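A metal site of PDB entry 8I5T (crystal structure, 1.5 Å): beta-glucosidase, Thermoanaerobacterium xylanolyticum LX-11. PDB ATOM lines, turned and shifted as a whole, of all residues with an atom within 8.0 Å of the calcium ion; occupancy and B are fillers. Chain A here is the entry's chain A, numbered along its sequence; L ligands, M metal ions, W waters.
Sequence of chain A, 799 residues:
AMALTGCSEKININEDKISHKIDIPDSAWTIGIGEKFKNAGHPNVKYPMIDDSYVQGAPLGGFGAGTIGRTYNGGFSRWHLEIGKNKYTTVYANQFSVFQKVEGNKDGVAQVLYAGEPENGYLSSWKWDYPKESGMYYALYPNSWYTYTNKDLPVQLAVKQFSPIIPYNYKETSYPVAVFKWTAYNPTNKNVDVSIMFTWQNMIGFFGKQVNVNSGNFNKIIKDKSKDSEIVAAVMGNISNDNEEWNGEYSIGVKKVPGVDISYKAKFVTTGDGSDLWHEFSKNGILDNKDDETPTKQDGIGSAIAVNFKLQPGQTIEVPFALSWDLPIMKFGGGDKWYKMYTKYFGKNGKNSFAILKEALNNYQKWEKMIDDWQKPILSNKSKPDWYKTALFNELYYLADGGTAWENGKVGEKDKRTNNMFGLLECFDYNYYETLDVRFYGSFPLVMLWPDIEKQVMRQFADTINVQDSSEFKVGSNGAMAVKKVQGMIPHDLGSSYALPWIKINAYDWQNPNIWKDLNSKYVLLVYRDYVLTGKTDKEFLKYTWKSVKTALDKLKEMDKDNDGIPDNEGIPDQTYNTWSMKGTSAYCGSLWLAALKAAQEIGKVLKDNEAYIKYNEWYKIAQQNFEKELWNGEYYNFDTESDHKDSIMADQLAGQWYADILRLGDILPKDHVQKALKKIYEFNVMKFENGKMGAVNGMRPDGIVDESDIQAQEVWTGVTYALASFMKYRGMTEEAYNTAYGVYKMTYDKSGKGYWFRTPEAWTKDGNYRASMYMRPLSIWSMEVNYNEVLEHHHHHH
OG1 of Thr 585 lies within hydrogen-bond range of OD2 of Asp 564 (3.0 Å).
The side-chain carboxylate of Asp 564 lies close to the side-chain carboxylate of Glu 630.
The side-chain amide nitrogen (ND2) of Asn 626 lies within hydrogen-bond range of the backbone carbonyl oxygen (O) of Asp 564 (2.8 Å).
OD1 of Asp 568 sits close to N of Lys 561 (2.9 Å).
N of Asp 568 sits at hydrogen-bond distance from O of Met 559.
The side-chain carboxylate of Asp 560 sits close to the backbone NH of Asn 563 (3.1 Å).
N of Gly 565 sits at hydrogen-bond distance from OD2 of Asp 560, at 2.9 Å.
Water W1 lies within hydrogen-bond range of the side-chain hydroxyl of Thr 585 (2.7 Å), the backbone carbonyl oxygen of Pro 567 (3.3 Å) and the side-chain carboxylate of Asp 568 (3.4 Å).
The calcium ion is bound by OD1 of Asp 564, OD1 of Asp 568, O of Ile 566, water W1, OD1 of Asp 560 and OD1 of Asp 562.
Slightly farther from the calcium ion lies an oxygen (O3) of the ligand (3.0 Å).
Within 4 Å of the calcium ion: Asp 560, Asp 562, Asp 564, Ile 566 and Asp 568.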
ATOM      1  N   LYS A 557      15.698  -7.851  14.286  1.00  0.00           N
ATOM      2  CA  LYS A 557      16.718  -7.690  15.345  1.00  0.00           C
ATOM      3  C   LYS A 557      17.107  -6.225  15.524  1.00  0.00           C
ATOM      4  O   LYS A 557      17.369  -5.791  16.636  1.00  0.00           O
ATOM      5  CB  LYS A 557      17.950  -8.544  15.021  1.00  0.00           C
ATOM      6  CG  LYS A 557      19.074  -8.530  16.063  1.00  0.00           C
ATOM      7  CD  LYS A 557      18.630  -9.118  17.399  1.00  0.00           C
ATOM      8  CE  LYS A 557      19.795  -9.592  18.249  1.00  0.00           C
ATOM      9  NZ  LYS A 557      20.743  -8.498  18.593  1.00  0.00           N
ATOM     10  N   MET A 559      15.234  -3.753  15.558  1.00  0.00           N
ATOM     11  CA  MET A 559      14.203  -3.070  16.350  1.00  0.00           C
ATOM     12  C   MET A 559      14.333  -3.318  17.860  1.00  0.00           C
ATOM     13  O   MET A 559      13.500  -2.865  18.637  1.00  0.00           O
ATOM     14  CB  MET A 559      12.825  -3.467  15.852  1.00  0.00           C
ATOM     15  CG  MET A 559      12.609  -3.103  14.394  1.00  0.00           C
ATOM     16  SD  MET A 559      11.037  -3.741  13.782  1.00  0.00           S
ATOM     17  CE  MET A 559      10.990  -3.012  12.139  1.00  0.00           C
ATOM     18  N   ASP A 560      15.371  -4.028  18.263  1.00  0.00           N
ATOM     19  CA  ASP A 560      15.733  -4.139  19.680  1.00  0.00           C
ATOM     20  C   ASP A 560      16.439  -2.853  20.103  1.00  0.00           C
ATOM     21  O   ASP A 560      17.596  -2.674  19.795  1.00  0.00           O
ATOM     22  CB  ASP A 560      16.641  -5.361  19.857  1.00  0.00           C
ATOM     23  CG  ASP A 560      17.156  -5.532  21.261  1.00  0.00           C
ATOM     24  OD1 ASP A 560      16.580  -4.966  22.210  1.00  0.00           O
ATOM     25  OD2 ASP A 560      18.152  -6.266  21.402  1.00  0.00           O
ATOM     26  N   LYS A 561      15.744  -1.982  20.823  1.00  0.00           N
ATOM     27  CA  LYS A 561      16.288  -0.670  21.235  1.00  0.00           C
ATOM     28  C   LYS A 561      17.269  -0.767  22.402  1.00  0.00           C
ATOM     29  O   LYS A 561      18.320  -0.134  22.387  1.00  0.00           O
ATOM     30  CB  LYS A 561      15.163   0.279  21.624  1.00  0.00           C
ATOM     31  CG  LYS A 561      14.255   0.667  20.467  1.00  0.00           C
ATOM     32  CD  LYS A 561      13.022   1.422  20.972  1.00  0.00           C
ATOM     33  CE  LYS A 561      12.312   2.136  19.839  1.00  0.00           C
ATOM     34  NZ  LYS A 561      11.091   2.854  20.325  1.00  0.00           N
ATOM     35  N   ASP A 562      16.908  -1.564  23.401  1.00  0.00           N
ATOM     36  CA  ASP A 562      17.642  -1.612  24.680  1.00  0.00           C
ATOM     37  C   ASP A 562      18.617  -2.792  24.823  1.00  0.00           C
ATOM     38  O   ASP A 562      19.130  -3.056  25.913  1.00  0.00           O
ATOM     39  CB  ASP A 562      16.637  -1.608  25.834  1.00  0.00           C
ATOM     40  CG  ASP A 562      15.860  -2.913  25.937  1.00  0.00           C
ATOM     41  OD1 ASP A 562      15.731  -3.626  24.909  1.00  0.00           O
ATOM     42  OD2 ASP A 562      15.380  -3.219  27.039  1.00  0.00           O
ATOM     43  N   ASN A 563      18.852  -3.511  23.730  1.00  0.00           N
ATOM     44  CA  ASN A 563      19.835  -4.592  23.666  1.00  0.00           C
ATOM     45  C   ASN A 563      19.612  -5.797  24.608  1.00  0.00           C
ATOM     46  O   ASN A 563      20.586  -6.435  25.041  1.00  0.00           O
ATOM     47  CB  ASN A 563      21.264  -4.038  23.798  1.00  0.00           C
ATOM     48  CG  ASN A 563      22.151  -4.512  22.685  1.00  0.00           C
ATOM     49  OD1 ASN A 563      22.125  -3.949  21.591  1.00  0.00           O
ATOM     50  ND2 ASN A 563      22.912  -5.582  22.925  1.00  0.00           N
ATOM     51  N   ASP A 564      18.342  -6.127  24.881  1.00  0.00           N
ATOM     52  CA  ASP A 564      18.011  -7.376  25.602  1.00  0.00           C
ATOM     53  C   ASP A 564      17.843  -8.582  24.654  1.00  0.00           C
ATOM     54  O   ASP A 564      17.494  -9.673  25.099  1.00  0.00           O
ATOM     55  CB  ASP A 564      16.769  -7.188  26.491  1.00  0.00           C
ATOM     56  CG  ASP A 564      15.449  -7.123  25.685  1.00  0.00           C
ATOM     57  OD1 ASP A 564      15.484  -6.908  24.458  1.00  0.00           O
ATOM     58  OD2 ASP A 564      14.381  -7.233  26.288  1.00  0.00           O
ATOM     59  N   GLY A 565      18.066  -8.368  23.356  1.00  0.00           N
ATOM     60  CA  GLY A 565      18.015  -9.424  22.355  1.00  0.00           C
ATOM     61  C   GLY A 565      16.624  -9.620  21.728  1.00  0.00           C
ATOM     62  O   GLY A 565      16.470 -10.507  20.898  1.00  0.00           O
ATOM     63  N   ILE A 566      15.672  -8.776  22.096  1.00  0.00           N
ATOM     64  CA  ILE A 566      14.252  -8.940  21.725  1.00  0.00           C
ATOM     65  C   ILE A 566      13.798  -7.636  21.064  1.00  0.00           C
ATOM     66  O   ILE A 566      14.060  -6.562  21.596  1.00  0.00           O
ATOM     67  CB  ILE A 566      13.358  -9.227  22.958  1.00  0.00           C
ATOM     68  CG1 ILE A 566      13.895 -10.455  23.728  1.00  0.00           C
ATOM     69  CG2 ILE A 566      11.910  -9.488  22.538  1.00  0.00           C
ATOM     70  CD1 ILE A 566      13.261 -10.686  25.063  1.00  0.00           C
ATOM     71  N   PRO A 567      13.105  -7.707  19.919  1.00  0.00           N
ATOM     72  CA  PRO A 567      12.554  -6.449  19.394  1.00  0.00           C
ATOM     73  C   PRO A 567      11.605  -5.761  20.372  1.00  0.00           C
ATOM     74  O   PRO A 567      10.860  -6.436  21.087  1.00  0.00           O
ATOM     75  CB  PRO A 567      11.816  -6.885  18.117  1.00  0.00           C
ATOM     76  CG  PRO A 567      11.605  -8.341  18.268  1.00  0.00           C
ATOM     77  CD  PRO A 567      12.762  -8.858  19.059  1.00  0.00           C
ATOM     78  N   ASP A 568      11.667  -4.423  20.439  1.00  0.00           N
ATOM     79  CA  ASP A 568      10.822  -3.641  21.348  1.00  0.00           C
ATOM     80  C   ASP A 568       9.531  -3.229  20.692  1.00  0.00           C
ATOM     81  O   ASP A 568       9.557  -2.579  19.632  1.00  0.00           O
ATOM     82  CB  ASP A 568      11.531  -2.363  21.794  1.00  0.00           C
ATOM     83  CG  ASP A 568      12.649  -2.625  22.749  1.00  0.00           C
ATOM     84  OD1 ASP A 568      13.651  -3.240  22.335  1.00  0.00           O
ATOM     85  OD2 ASP A 568      12.493  -2.250  23.942  1.00  0.00           O
ATOM     86  N   ASN A 569       8.400  -3.532  21.328  1.00  0.00           N
ATOM     87  CA  ASN A 569       7.138  -2.917  20.902  1.00  0.00           C
ATOM     88  C   ASN A 569       7.182  -1.441  21.335  1.00  0.00           C
ATOM     89  O   ASN A 569       7.769  -1.116  22.367  1.00  0.00           O
ATOM     90  CB  ASN A 569       5.918  -3.630  21.504  1.00  0.00           C
ATOM     91  CG  ASN A 569       5.726  -5.025  20.960  1.00  0.00           C
ATOM     92  OD1 ASN A 569       6.132  -6.018  21.589  1.00  0.00           O
ATOM     93  ND2 ASN A 569       5.087  -5.131  19.802  1.00  0.00           N
ATOM     94  N   GLY A 584       7.749  -2.291  25.036  1.00  0.00           N
ATOM     95  CA  GLY A 584       8.887  -3.034  25.550  1.00  0.00           C
ATOM     96  C   GLY A 584       8.892  -4.445  25.011  1.00  0.00           C
ATOM     97  O   GLY A 584       8.658  -4.662  23.818  1.00  0.00           O
ATOM     98  N   THR A 585       9.157  -5.400  25.885  1.00  0.00           N
ATOM     99  CA  THR A 585       9.103  -6.810  25.513  1.00  0.00           C
ATOM    100  C   THR A 585       7.698  -7.267  25.841  1.00  0.00           C
ATOM    101  O   THR A 585       7.231  -7.090  26.945  1.00  0.00           O
ATOM    102  CB  THR A 585      10.120  -7.645  26.297  1.00  0.00           C
ATOM    103  OG1 THR A 585      11.445  -7.265  25.890  1.00  0.00           O
ATOM    104  CG2 THR A 585       9.942  -9.120  26.002  1.00  0.00           C
ATOM    105  N   TRP A 593       9.028 -14.243  18.419  1.00  0.00           N
ATOM    106  CA  TRP A 593      10.450 -14.038  18.112  1.00  0.00           C
ATOM    107  C   TRP A 593      11.316 -15.233  18.519  1.00  0.00           C
ATOM    108  O   TRP A 593      12.105 -15.745  17.725  1.00  0.00           O
ATOM    109  CB  TRP A 593      10.903 -12.758  18.794  1.00  0.00           C
ATOM    110  CG  TRP A 593      12.396 -12.425  18.761  1.00  0.00           C
ATOM    111  CD1 TRP A 593      13.231 -12.349  19.850  1.00  0.00           C
ATOM    112  CD2 TRP A 593      13.193 -12.106  17.623  1.00  0.00           C
ATOM    113  NE1 TRP A 593      14.497 -11.990  19.457  1.00  0.00           N
ATOM    114  CE2 TRP A 593      14.509 -11.858  18.095  1.00  0.00           C
ATOM    115  CE3 TRP A 593      12.939 -12.014  16.260  1.00  0.00           C
ATOM    116  CZ2 TRP A 593      15.554 -11.517  17.227  1.00  0.00           C
ATOM    117  CZ3 TRP A 593      13.969 -11.686  15.403  1.00  0.00           C
ATOM    118  CH2 TRP A 593      15.270 -11.422  15.898  1.00  0.00           C
ATOM    119  N   ASN A 626      16.327 -13.555  28.704  1.00  0.00           N
ATOM    120  CA  ASN A 626      15.759 -12.264  29.041  1.00  0.00           C
ATOM    121  C   ASN A 626      14.226 -12.222  29.035  1.00  0.00           C
ATOM    122  O   ASN A 626      13.625 -11.568  29.886  1.00  0.00           O
ATOM    123  CB  ASN A 626      16.345 -11.187  28.134  1.00  0.00           C
ATOM    124  CG  ASN A 626      17.757 -10.801  28.547  1.00  0.00           C
ATOM    125  OD1 ASN A 626      18.097 -10.875  29.729  1.00  0.00           O
ATOM    126  ND2 ASN A 626      18.563 -10.390  27.594  1.00  0.00           N
ATOM    127  N   GLU A 630      12.201 -11.023  32.337  1.00  0.00           N
ATOM    128  CA  GLU A 630      11.358  -9.858  32.202  1.00  0.00           C
ATOM    129  C   GLU A 630       9.866 -10.120  32.439  1.00  0.00           C
ATOM    130  O   GLU A 630       9.177  -9.249  32.956  1.00  0.00           O
ATOM    131  CB  GLU A 630      11.526  -9.232  30.823  1.00  0.00           C
ATOM    132  CG  GLU A 630      12.878  -8.555  30.620  1.00  0.00           C
ATOM    133  CD  GLU A 630      13.193  -8.323  29.157  1.00  0.00           C
ATOM    134  OE1 GLU A 630      12.253  -8.394  28.324  1.00  0.00           O
ATOM    135  OE2 GLU A 630      14.380  -8.091  28.841  1.00  0.00           O
ATOM    136  N   THR A 641       6.408  -5.405  29.293  1.00  0.00           N
ATOM    137  CA  THR A 641       7.262  -4.804  30.341  1.00  0.00           C
ATOM    138  C   THR A 641       6.994  -3.335  30.655  1.00  0.00           C
ATOM    139  O   THR A 641       7.460  -2.846  31.699  1.00  0.00           O
ATOM    140  CB  THR A 641       8.745  -4.947  29.975  1.00  0.00           C
ATOM    141  OG1 THR A 641       8.979  -4.350  28.683  1.00  0.00           O
ATOM    142  CG2 THR A 641       9.152  -6.411  29.944  1.00  0.00           C
ATOM    143  N   GLU A 642       6.306  -2.609  29.778  1.00  0.00           N
ATOM    144  CA  GLU A 642       6.209  -1.139  29.898  1.00  0.00           C
ATOM    145  C   GLU A 642       4.823  -0.495  29.803  1.00  0.00           C
ATOM    146  O   GLU A 642       4.706   0.701  30.067  1.00  0.00           O
ATOM    147  CB  GLU A 642       7.164  -0.467  28.897  1.00  0.00           C
ATOM    148  CG  GLU A 642       8.640  -0.758  29.146  1.00  0.00           C
ATOM    149  CD  GLU A 642       9.577  -0.120  28.119  1.00  0.00           C
ATOM    150  OE1 GLU A 642       9.266   0.990  27.646  1.00  0.00           O
ATOM    151  OE2 GLU A 642      10.618  -0.718  27.797  1.00  0.00           O
HETATM  152  C1  LIG L   1      12.828  -4.929  29.017  1.00  0.00           C
HETATM  153  O1  LIG L   1      12.987  -4.604  30.405  1.00  0.00           O
HETATM  154  C2  LIG L   1      12.427  -3.674  28.226  1.00  0.00           C
HETATM  155  O2  LIG L   1      11.236  -3.087  28.770  1.00  0.00           O
HETATM  156  C3  LIG L   1      12.138  -4.027  26.772  1.00  0.00           C
HETATM  157  O3  LIG L   1      13.304  -4.241  25.987  1.00  0.00           O
HETATM  158 CA    CA M   1      14.499  -5.130  23.394  1.00  0.00          CA
HETATM  159  O   HOH W   1      12.227  -5.607  23.923  1.00  0.00           O
